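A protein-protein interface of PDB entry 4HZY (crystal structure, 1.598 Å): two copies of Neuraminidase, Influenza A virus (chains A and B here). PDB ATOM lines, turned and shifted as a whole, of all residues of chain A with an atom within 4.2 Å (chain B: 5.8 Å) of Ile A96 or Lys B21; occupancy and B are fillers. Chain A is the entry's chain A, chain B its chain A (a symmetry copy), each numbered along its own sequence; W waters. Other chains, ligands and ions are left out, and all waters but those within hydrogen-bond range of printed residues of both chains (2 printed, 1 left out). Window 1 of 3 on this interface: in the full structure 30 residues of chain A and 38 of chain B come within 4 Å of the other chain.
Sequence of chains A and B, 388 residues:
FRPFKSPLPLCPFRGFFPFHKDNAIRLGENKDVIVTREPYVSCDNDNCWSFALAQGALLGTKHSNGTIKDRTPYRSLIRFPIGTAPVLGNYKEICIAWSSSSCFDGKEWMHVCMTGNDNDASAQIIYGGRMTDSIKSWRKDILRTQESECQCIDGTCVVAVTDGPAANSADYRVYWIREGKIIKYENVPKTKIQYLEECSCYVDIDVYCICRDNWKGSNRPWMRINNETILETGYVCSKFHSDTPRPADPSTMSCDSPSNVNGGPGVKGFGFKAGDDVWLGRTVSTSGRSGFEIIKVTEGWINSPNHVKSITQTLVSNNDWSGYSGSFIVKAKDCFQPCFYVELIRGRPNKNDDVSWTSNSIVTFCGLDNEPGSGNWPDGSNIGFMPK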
ATOM      1  N   PRO A  73      17.573  23.635 -14.946  1.00  0.00           N
ATOM      2  CA  PRO A  73      17.875  23.490 -13.516  1.00  0.00           C
ATOM      3  C   PRO A  73      19.374  23.444 -13.239  1.00  0.00           C
ATOM      4  O   PRO A  73      19.772  23.466 -12.081  1.00  0.00           O
ATOM      5  CB  PRO A  73      17.273  22.129 -13.159  1.00  0.00           C
ATOM      6  CG  PRO A  73      16.355  21.768 -14.307  1.00  0.00           C
ATOM      7  CD  PRO A  73      16.932  22.434 -15.513  1.00  0.00           C
ATOM      8  N   TYR A  74      20.192  23.380 -14.287  1.00  0.00           N
ATOM      9  CA  TYR A  74      21.638  23.204 -14.118  1.00  0.00           C
ATOM     10  C   TYR A  74      22.351  24.540 -14.189  1.00  0.00           C
ATOM     11  O   TYR A  74      23.580  24.588 -14.219  1.00  0.00           O
ATOM     12  CB  TYR A  74      22.178  22.234 -15.175  1.00  0.00           C
ATOM     13  CG  TYR A  74      21.215  21.088 -15.355  1.00  0.00           C
ATOM     14  CD1 TYR A  74      20.918  20.248 -14.288  1.00  0.00           C
ATOM     15  CD2 TYR A  74      20.558  20.875 -16.560  1.00  0.00           C
ATOM     16  CE1 TYR A  74      20.013  19.228 -14.418  1.00  0.00           C
ATOM     17  CE2 TYR A  74      19.651  19.834 -16.699  1.00  0.00           C
ATOM     18  CZ  TYR A  74      19.378  19.028 -15.621  1.00  0.00           C
ATOM     19  OH  TYR A  74      18.478  17.977 -15.736  1.00  0.00           O
ATOM     20  N   ARG A  75      21.582  25.625 -14.239  1.00  0.00           N
ATOM     21  CA  ARG A  75      22.166  26.960 -14.229  1.00  0.00           C
ATOM     22  C   ARG A  75      22.283  27.471 -12.802  1.00  0.00           C
ATOM     23  O   ARG A  75      21.355  27.302 -11.993  1.00  0.00           O
ATOM     24  CB  ARG A  75      21.357  27.933 -15.097  1.00  0.00           C
ATOM     25  CG  ARG A  75      21.300  27.503 -16.559  1.00  0.00           C
ATOM     26  CD  ARG A  75      20.976  28.693 -17.447  1.00  0.00           C
ATOM     27  NE  ARG A  75      22.164  29.526 -17.658  1.00  0.00           N
ATOM     28  CZ  ARG A  75      22.197  30.561 -18.486  1.00  0.00           C
ATOM     29  NH1 ARG A  75      21.096  30.912 -19.133  1.00  0.00           N
ATOM     30  NH2 ARG A  75      23.322  31.247 -18.657  1.00  0.00           N
ATOM     31  N   SER A  76      23.446  28.042 -12.496  1.00  0.00           N
ATOM     32  CA  SER A  76      23.726  28.634 -11.192  1.00  0.00           C
ATOM     33  C   SER A  76      24.342  29.993 -11.405  1.00  0.00           C
ATOM     34  O   SER A  76      25.096  30.183 -12.348  1.00  0.00           O
ATOM     35  CB  SER A  76      24.760  27.802 -10.434  1.00  0.00           C
ATOM     36  OG  SER A  76      24.191  26.631  -9.880  1.00  0.00           O
ATOM     37  N   GLU A  93      29.921  29.212  -6.235  1.00  0.00           N
ATOM     38  CA  GLU A  93      28.528  29.087  -6.628  1.00  0.00           C
ATOM     39  C   GLU A  93      27.691  29.868  -5.627  1.00  0.00           C
ATOM     40  O   GLU A  93      27.754  29.617  -4.422  1.00  0.00           O
ATOM     41  CB  GLU A  93      28.076  27.622  -6.678  1.00  0.00           C
ATOM     42  CG  GLU A  93      26.766  27.440  -7.479  1.00  0.00           C
ATOM     43  CD  GLU A  93      25.574  26.982  -6.651  1.00  0.00           C
ATOM     44  OE1 GLU A  93      25.684  26.905  -5.411  1.00  0.00           O
ATOM     45  OE2 GLU A  93      24.514  26.697  -7.251  1.00  0.00           O
ATOM     46  N   CYS A  95      24.119  30.622  -5.978  1.00  0.00           N
ATOM     47  CA  CYS A  95      22.795  30.030  -5.817  1.00  0.00           C
ATOM     48  C   CYS A  95      22.377  29.411  -7.131  1.00  0.00           C
ATOM     49  O   CYS A  95      22.937  29.722  -8.174  1.00  0.00           O
ATOM     50  CB  CYS A  95      21.779  31.111  -5.471  1.00  0.00           C
ATOM     51  SG  CYS A  95      21.789  32.416  -6.731  1.00  0.00           S
ATOM     52  N   ILE A  96      21.369  28.550  -7.076  1.00  0.00           N
ATOM     53  CA  ILE A  96      20.776  27.999  -8.283  1.00  0.00           C
ATOM     54  C   ILE A  96      19.990  29.130  -8.930  1.00  0.00           C
ATOM     55  O   ILE A  96      19.195  29.775  -8.260  1.00  0.00           O
ATOM     56  CB  ILE A  96      19.828  26.838  -7.921  1.00  0.00           C
ATOM     57  CG1 ILE A  96      20.608  25.738  -7.191  1.00  0.00           C
ATOM     58  CG2 ILE A  96      19.168  26.261  -9.178  1.00  0.00           C
ATOM     59  CD1 ILE A  96      19.729  24.717  -6.501  1.00  0.00           C
ATOM     60  N   ALA A  97      20.216  29.391 -10.218  1.00  0.00           N
ATOM     61  CA  ALA A  97      19.567  30.531 -10.864  1.00  0.00           C
ATOM     62  C   ALA A  97      19.609  30.472 -12.382  1.00  0.00           C
ATOM     63  O   ALA A  97      20.669  30.223 -12.970  1.00  0.00           O
ATOM     64  CB  ALA A  97      20.220  31.864 -10.405  1.00  0.00           C
ATOM     65  N   CYS A 113      17.830  35.208  -6.887  1.00  0.00           N
ATOM     66  CA  CYS A 113      18.054  34.048  -7.765  1.00  0.00           C
ATOM     67  C   CYS A 113      16.746  33.381  -8.163  1.00  0.00           C
ATOM     68  O   CYS A 113      16.057  32.828  -7.314  1.00  0.00           O
ATOM     69  CB  CYS A 113      18.904  33.020  -7.025  1.00  0.00           C
ATOM     70  SG  CYS A 113      20.358  33.752  -6.214  1.00  0.00           S
ATOM     71  N   THR A 115      14.707  30.368 -10.069  1.00  0.00           N
ATOM     72  CA  THR A 115      14.844  29.066 -10.705  1.00  0.00           C
ATOM     73  C   THR A 115      13.525  28.307 -10.593  1.00  0.00           C
ATOM     74  O   THR A 115      12.578  28.792  -9.965  1.00  0.00           O
ATOM     75  CB  THR A 115      16.041  28.245 -10.129  1.00  0.00           C
ATOM     76  OG1 THR A 115      16.146  26.986 -10.813  1.00  0.00           O
ATOM     77  CG2 THR A 115      15.839  27.991  -8.640  1.00  0.00           C
ATOM     78  N   PRO B  18      15.067  26.075  -3.425  1.00  0.00           N
ATOM     79  CA  PRO B  18      16.362  25.643  -3.963  1.00  0.00           C
ATOM     80  C   PRO B  18      17.489  26.618  -3.627  1.00  0.00           C
ATOM     81  O   PRO B  18      17.339  27.827  -3.813  1.00  0.00           O
ATOM     82  CB  PRO B  18      16.117  25.580  -5.474  1.00  0.00           C
ATOM     83  CG  PRO B  18      14.989  26.527  -5.708  1.00  0.00           C
ATOM     84  CD  PRO B  18      14.109  26.423  -4.489  1.00  0.00           C
ATOM     85  N   PHE B  19      18.609  26.076  -3.146  1.00  0.00           N
ATOM     86  CA  PHE B  19      19.690  26.872  -2.558  1.00  0.00           C
ATOM     87  C   PHE B  19      20.922  26.773  -3.474  1.00  0.00           C
ATOM     88  O   PHE B  19      21.139  27.639  -4.339  1.00  0.00           O
ATOM     89  CB  PHE B  19      19.969  26.296  -1.158  1.00  0.00           C
ATOM     90  CG  PHE B  19      20.822  27.154  -0.251  1.00  0.00           C
ATOM     91  CD1 PHE B  19      20.986  28.512  -0.445  1.00  0.00           C
ATOM     92  CD2 PHE B  19      21.464  26.557   0.828  1.00  0.00           C
ATOM     93  CE1 PHE B  19      21.777  29.268   0.448  1.00  0.00           C
ATOM     94  CE2 PHE B  19      22.248  27.302   1.705  1.00  0.00           C
ATOM     95  CZ  PHE B  19      22.399  28.653   1.512  1.00  0.00           C
ATOM     96  N   HIS B  20      21.706  25.710  -3.294  1.00  0.00           N
ATOM     97  CA  HIS B  20      22.957  25.505  -4.040  1.00  0.00           C
ATOM     98  C   HIS B  20      22.887  24.173  -4.794  1.00  0.00           C
ATOM     99  O   HIS B  20      22.291  23.219  -4.315  1.00  0.00           O
ATOM    100  CB  HIS B  20      24.153  25.440  -3.072  1.00  0.00           C
ATOM    101  CG  HIS B  20      24.536  26.753  -2.448  1.00  0.00           C
ATOM    102  ND1 HIS B  20      25.381  27.660  -3.058  1.00  0.00           N
ATOM    103  CD2 HIS B  20      24.237  27.277  -1.236  1.00  0.00           C
ATOM    104  CE1 HIS B  20      25.562  28.696  -2.260  1.00  0.00           C
ATOM    105  NE2 HIS B  20      24.876  28.498  -1.148  1.00  0.00           N
ATOM    106  N   LYS B  21      23.500  24.097  -5.973  1.00  0.00           N
ATOM    107  CA  LYS B  21      23.560  22.842  -6.724  1.00  0.00           C
ATOM    108  C   LYS B  21      24.902  22.764  -7.409  1.00  0.00           C
ATOM    109  O   LYS B  21      25.290  23.711  -8.086  1.00  0.00           O
ATOM    110  CB  LYS B  21      22.464  22.797  -7.793  1.00  0.00           C
ATOM    111  CG  LYS B  21      22.357  21.462  -8.527  1.00  0.00           C
ATOM    112  CD  LYS B  21      21.273  21.546  -9.595  1.00  0.00           C
ATOM    113  CE  LYS B  21      20.943  20.166 -10.198  1.00  0.00           C
ATOM    114  NZ  LYS B  21      22.166  19.462 -10.688  1.00  0.00           N
ATOM    115  N   ASP B  22      25.606  21.645  -7.276  1.00  0.00           N
ATOM    116  CA  ASP B  22      26.957  21.647  -7.814  1.00  0.00           C
ATOM    117  C   ASP B  22      27.138  21.115  -9.231  1.00  0.00           C
ATOM    118  O   ASP B  22      28.135  21.419  -9.862  1.00  0.00           O
ATOM    119  CB  ASP B  22      27.991  21.065  -6.840  1.00  0.00           C
ATOM    120  CG  ASP B  22      27.771  19.616  -6.526  1.00  0.00           C
ATOM    121  OD1 ASP B  22      27.115  18.906  -7.306  1.00  0.00           O
ATOM    122  OD2 ASP B  22      28.314  19.164  -5.492  1.00  0.00           O
ATOM    123  N   ASN B  23      26.186  20.339  -9.736  1.00  0.00           N
ATOM    124  CA  ASN B  23      26.313  19.825 -11.104  1.00  0.00           C
ATOM    125  C   ASN B  23      27.654  19.110 -11.303  1.00  0.00           C
ATOM    126  O   ASN B  23      28.252  19.156 -12.375  1.00  0.00           O
ATOM    127  CB  ASN B  23      26.170  20.985 -12.102  1.00  0.00           C
ATOM    128  CG  ASN B  23      24.825  21.678 -11.999  1.00  0.00           C
ATOM    129  OD1 ASN B  23      24.730  22.868 -11.627  1.00  0.00           O
ATOM    130  ND2 ASN B  23      23.774  20.947 -12.331  1.00  0.00           N
ATOM    131  N   ARG B  26      28.122  16.419 -14.330  1.00  0.00           N
ATOM    132  CA  ARG B  26      28.168  17.161 -15.593  1.00  0.00           C
ATOM    133  C   ARG B  26      29.527  17.834 -15.761  1.00  0.00           C
ATOM    134  O   ARG B  26      30.157  17.743 -16.817  1.00  0.00           O
ATOM    135  CB  ARG B  26      27.066  18.233 -15.639  1.00  0.00           C
ATOM    136  CG  ARG B  26      25.655  17.667 -15.749  1.00  0.00           C
ATOM    137  CD  ARG B  26      24.628  18.752 -15.505  1.00  0.00           C
ATOM    138  NE  ARG B  26      24.766  19.891 -16.415  1.00  0.00           N
ATOM    139  CZ  ARG B  26      24.158  19.989 -17.591  1.00  0.00           C
ATOM    140  NH1 ARG B  26      24.329  21.071 -18.344  1.00  0.00           N
ATOM    141  NH2 ARG B  26      23.373  19.009 -18.014  1.00  0.00           N
ATOM    142  N   GLY B  83      28.192  24.203  -3.255  1.00  0.00           N
ATOM    143  CA  GLY B  83      27.684  24.330  -4.610  1.00  0.00           C
ATOM    144  C   GLY B  83      28.748  24.264  -5.693  1.00  0.00           C
ATOM    145  O   GLY B  83      28.413  24.326  -6.869  1.00  0.00           O
ATOM    146  N   THR B  84      30.023  24.144  -5.326  1.00  0.00           N
ATOM    147  CA  THR B  84      31.050  23.879  -6.342  1.00  0.00           C
ATOM    148  C   THR B  84      31.339  22.381  -6.509  1.00  0.00           C
ATOM    149  O   THR B  84      31.079  21.566  -5.611  1.00  0.00           O
ATOM    150  CB  THR B  84      32.381  24.632  -6.088  1.00  0.00           C
ATOM    151  OG1 THR B  84      33.070  24.069  -4.956  1.00  0.00           O
ATOM    152  CG2 THR B  84      32.115  26.134  -5.874  1.00  0.00           C
ATOM    153  N   LEU B 344      22.915  12.949  -5.135  1.00  0.00           N
ATOM    154  CA  LEU B 344      22.404  12.432  -6.397  1.00  0.00           C
ATOM    155  C   LEU B 344      23.439  11.468  -6.965  1.00  0.00           C
ATOM    156  O   LEU B 344      24.436  11.886  -7.554  1.00  0.00           O
ATOM    157  CB  LEU B 344      22.116  13.592  -7.358  1.00  0.00           C
ATOM    158  CG  LEU B 344      21.271  14.717  -6.746  1.00  0.00           C
ATOM    159  CD1 LEU B 344      21.278  15.976  -7.612  1.00  0.00           C
ATOM    160  CD2 LEU B 344      19.837  14.239  -6.510  1.00  0.00           C
ATOM    161  N   SER B 361      26.494  14.019  -7.323  1.00  0.00           N
ATOM    162  CA  SER B 361      26.454  15.465  -7.201  1.00  0.00           C
ATOM    163  C   SER B 361      25.560  15.808  -6.018  1.00  0.00           C
ATOM    164  O   SER B 361      25.103  14.926  -5.307  1.00  0.00           O
ATOM    165  CB  SER B 361      25.985  16.122  -8.504  1.00  0.00           C
ATOM    166  OG  SER B 361      24.635  15.798  -8.775  1.00  0.00           O
ATOM    167  N   ILE B 362      25.362  17.097  -5.784  1.00  0.00           N
ATOM    168  CA  ILE B 362      24.628  17.566  -4.619  1.00  0.00           C
ATOM    169  C   ILE B 362      23.620  18.627  -5.030  1.00  0.00           C
ATOM    170  O   ILE B 362      23.902  19.450  -5.905  1.00  0.00           O
ATOM    171  CB  ILE B 362      25.580  18.212  -3.593  1.00  0.00           C
ATOM    172  CG1 ILE B 362      26.717  17.255  -3.237  1.00  0.00           C
ATOM    173  CG2 ILE B 362      24.821  18.623  -2.338  1.00  0.00           C
ATOM    174  CD1 ILE B 362      27.736  17.839  -2.262  1.00  0.00           C
ATOM    175  N   VAL B 363      22.444  18.599  -4.407  1.00  0.00           N
ATOM    176  CA  VAL B 363      21.526  19.730  -4.465  1.00  0.00           C
ATOM    177  C   VAL B 363      21.049  20.028  -3.038  1.00  0.00           C
ATOM    178  O   VAL B 363      21.018  19.133  -2.201  1.00  0.00           O
ATOM    179  CB  VAL B 363      20.349  19.456  -5.443  1.00  0.00           C
ATOM    180  CG1 VAL B 363      19.505  18.267  -4.965  1.00  0.00           C
ATOM    181  CG2 VAL B 363      19.506  20.725  -5.642  1.00  0.00           C
ATOM    182  N   THR B 364      20.727  21.286  -2.749  1.00  0.00           N
ATOM    183  CA  THR B 364      20.350  21.681  -1.398  1.00  0.00           C
ATOM    184  C   THR B 364      19.143  22.596  -1.396  1.00  0.00           C
ATOM    185  O   THR B 364      18.901  23.323  -2.368  1.00  0.00           O
ATOM    186  CB  THR B 364      21.492  22.417  -0.670  1.00  0.00           C
ATOM    187  OG1 THR B 364      21.839  23.597  -1.402  1.00  0.00           O
ATOM    188  CG2 THR B 364      22.725  21.531  -0.529  1.00  0.00           C
ATOM    189  N   TRP B 377      15.279  19.433  -9.901  1.00  0.00           N
ATOM    190  CA  TRP B 377      16.710  19.732  -9.869  1.00  0.00           C
ATOM    191  C   TRP B 377      17.528  18.446  -9.713  1.00  0.00           C
ATOM    192  O   TRP B 377      18.157  18.212  -8.678  1.00  0.00           O
ATOM    193  CB  TRP B 377      17.025  20.756  -8.756  1.00  0.00           C
ATOM    194  CG  TRP B 377      16.355  22.096  -8.945  1.00  0.00           C
ATOM    195  CD1 TRP B 377      16.844  23.170  -9.636  1.00  0.00           C
ATOM    196  CD2 TRP B 377      15.070  22.492  -8.448  1.00  0.00           C
ATOM    197  NE1 TRP B 377      15.939  24.209  -9.598  1.00  0.00           N
ATOM    198  CE2 TRP B 377      14.844  23.815  -8.873  1.00  0.00           C
ATOM    199  CE3 TRP B 377      14.096  21.859  -7.675  1.00  0.00           C
ATOM    200  CZ2 TRP B 377      13.682  24.515  -8.551  1.00  0.00           C
ATOM    201  CZ3 TRP B 377      12.943  22.547  -7.360  1.00  0.00           C
ATOM    202  CH2 TRP B 377      12.743  23.863  -7.791  1.00  0.00           C
ATOM    203  N   PRO B 378      17.531  17.605 -10.762  1.00  0.00           N
ATOM    204  CA  PRO B 378      18.242  16.330 -10.711  1.00  0.00           C
ATOM    205  C   PRO B 378      19.706  16.509 -11.067  1.00  0.00           C
ATOM    206  O   PRO B 378      20.150  17.616 -11.382  1.00  0.00           O
ATOM    207  CB  PRO B 378      17.570  15.523 -11.816  1.00  0.00           C
ATOM    208  CG  PRO B 378      17.286  16.553 -12.847  1.00  0.00           C
ATOM    209  CD  PRO B 378      16.887  17.806 -12.071  1.00  0.00           C
ATOM    210  N   ASP B 379      20.453  15.413 -11.042  1.00  0.00           N
ATOM    211  CA  ASP B 379      21.874  15.481 -11.349  1.00  0.00           C
ATOM    212  C   ASP B 379      22.089  16.115 -12.719  1.00  0.00           C
ATOM    213  O   ASP B 379      22.939  16.990 -12.876  1.00  0.00           O
ATOM    214  CB  ASP B 379      22.473  14.090 -11.314  1.00  0.00           C
ATOM    215  CG  ASP B 379      23.871  14.063 -11.848  1.00  0.00           C
ATOM    216  OD1 ASP B 379      24.765  14.548 -11.127  1.00  0.00           O
ATOM    217  OD2 ASP B 379      24.062  13.582 -12.979  1.00  0.00           O
ATOM    218  N   GLY B 380      21.323  15.665 -13.709  1.00  0.00           N
ATOM    219  CA  GLY B 380      21.369  16.276 -15.027  1.00  0.00           C
ATOM    220  C   GLY B 380      22.424  15.784 -16.005  1.00  0.00           C
ATOM    221  O   GLY B 380      22.488  16.294 -17.124  1.00  0.00           O
HETATM  222  O   HOH W   1      26.476  24.994 -10.751  1.00  0.00           O
HETATM  223  O   HOH W   2      17.962  29.941  -5.714  1.00  0.00           O
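N of Ile A96 sits at hydrogen-bond distance from O of Phe B19 (2.9 Å). OE2 of Glu A93 lies within hydrogen-bond range of N of Lys B21. The side-chain carboxylate (OE1) of Glu A93 sits at hydrogen-bond distance from a ring nitrogen (ND1) of His B20. OG1 of Thr A115 sits at hydrogen-bond distance from NE1 of Trp B377 (3.0 Å). OD1 of Asn B23 sits close to O of Tyr A74 (3.3 Å).
N of Phe B19 is in hydrogen-bond range of O of Thr B364 (2.9 Å). The side-chain carboxylate (OD1) of Asp B379 is in hydrogen-bond range of the side-chain hydroxyl (OG) of Ser B361 (2.7 Å). OE2 of Glu A93 is in hydrogen-bond range of OG of Ser A76 (2.6 Å). The side-chain amino group of Lys B21 sits at hydrogen-bond distance from the backbone carbonyl oxygen of Pro B378 (2.8 Å). O of Asp B379 is in hydrogen-bond range of NZ of Lys B21 (3.4 Å). The guanidinium group of Arg B26 lies within hydrogen-bond range of the backbone carbonyl oxygen of Gly B380 (3.0 Å).
CD of Lys B21 touches O of Pro A73 (3.5 Å). Pro A73 touches Trp B377 (CB to CD1, 3.7 Å). Tyr A74 touches Lys B21. Tyr A74 touches Pro B378 (OH to CG, 3.4 Å). Tyr A74 touches Gly B380 (CE1 to CA, 3.3 Å). Ser A76 touches Lys B21 (OG to O, 3.6 Å). Glu A93 touches Thr B84 (N to CG2, 3.8 Å). Ile A96 touches Pro B18 (CD1 to CB, 3.9 Å). CG2 of Ile A96 touches NE1 of Trp B377, at 3.8 Å. CG2 of Thr A115 touches CG of Pro B18 (3.4 Å).
Of the printed residues of chain B, Tyr A74 touches Lys B21 (3.9 Å), Asn B23 (3.3 Å), Arg B26 (3.7 Å), Pro B378 (3.4 Å), Asp B379 (3.99 Å) and Gly B380 (3.3 Å). Of the printed residues of chain B, Ser A76 touches Lys B21 (3.6 Å). Ala A97 touches none of the printed residues of chain B. Of the printed residues of chain A, Phe B19 touches Cys A95 (3.3 Å) and Ile A96 (2.9 Å). Of chain A, only Pro A73, Tyr A74, Ser A76, Glu A93 and Ile A96 come within 4 Å of Lys B21. Of the printed residues of chain A, Trp B377 touches Pro A73, Ile A96 and Thr A115. The nearest printed residue of chain A that does not touch Asp B379 is Pro A73 (7.3 Å).
Of the 18 printed residues of chain B, 12 touch a printed residue of chain A. Hydrophobic or aromatic side chains of chain B within 4 Å of the printed part of chain A: Pro B18, His B20, Trp B377 and Pro B378. Of the 10 printed residues of chain A, 7 touch a printed residue of chain B. Printed residues of chain A that touch a printed residue of chain B: Pro A73, Tyr A74, Ser A76, Glu A93, Cys A95, Ile A96 and Thr A115. Among the printed residues, 21 pairs touch across the chains. Among the printed residues, no Asp or Glu carboxylate lies within 4 Å of a Lys or Arg side-chain nitrogen of the other chain.
No position is printed for both chains. Of the 21 pairs that touch across the chains among the printed residues, none has its exchanged pair printed and touching as well.
Water W2 bridges the backbone carbonyl oxygen (O) of Ile A96 (2.8 Å) and the backbone carbonyl oxygen (O) of Pro B18 (2.9 Å). Water W1 lies within hydrogen-bond range of OD1 of Asn B23, OG of Ser A76 and O of Lys B21.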
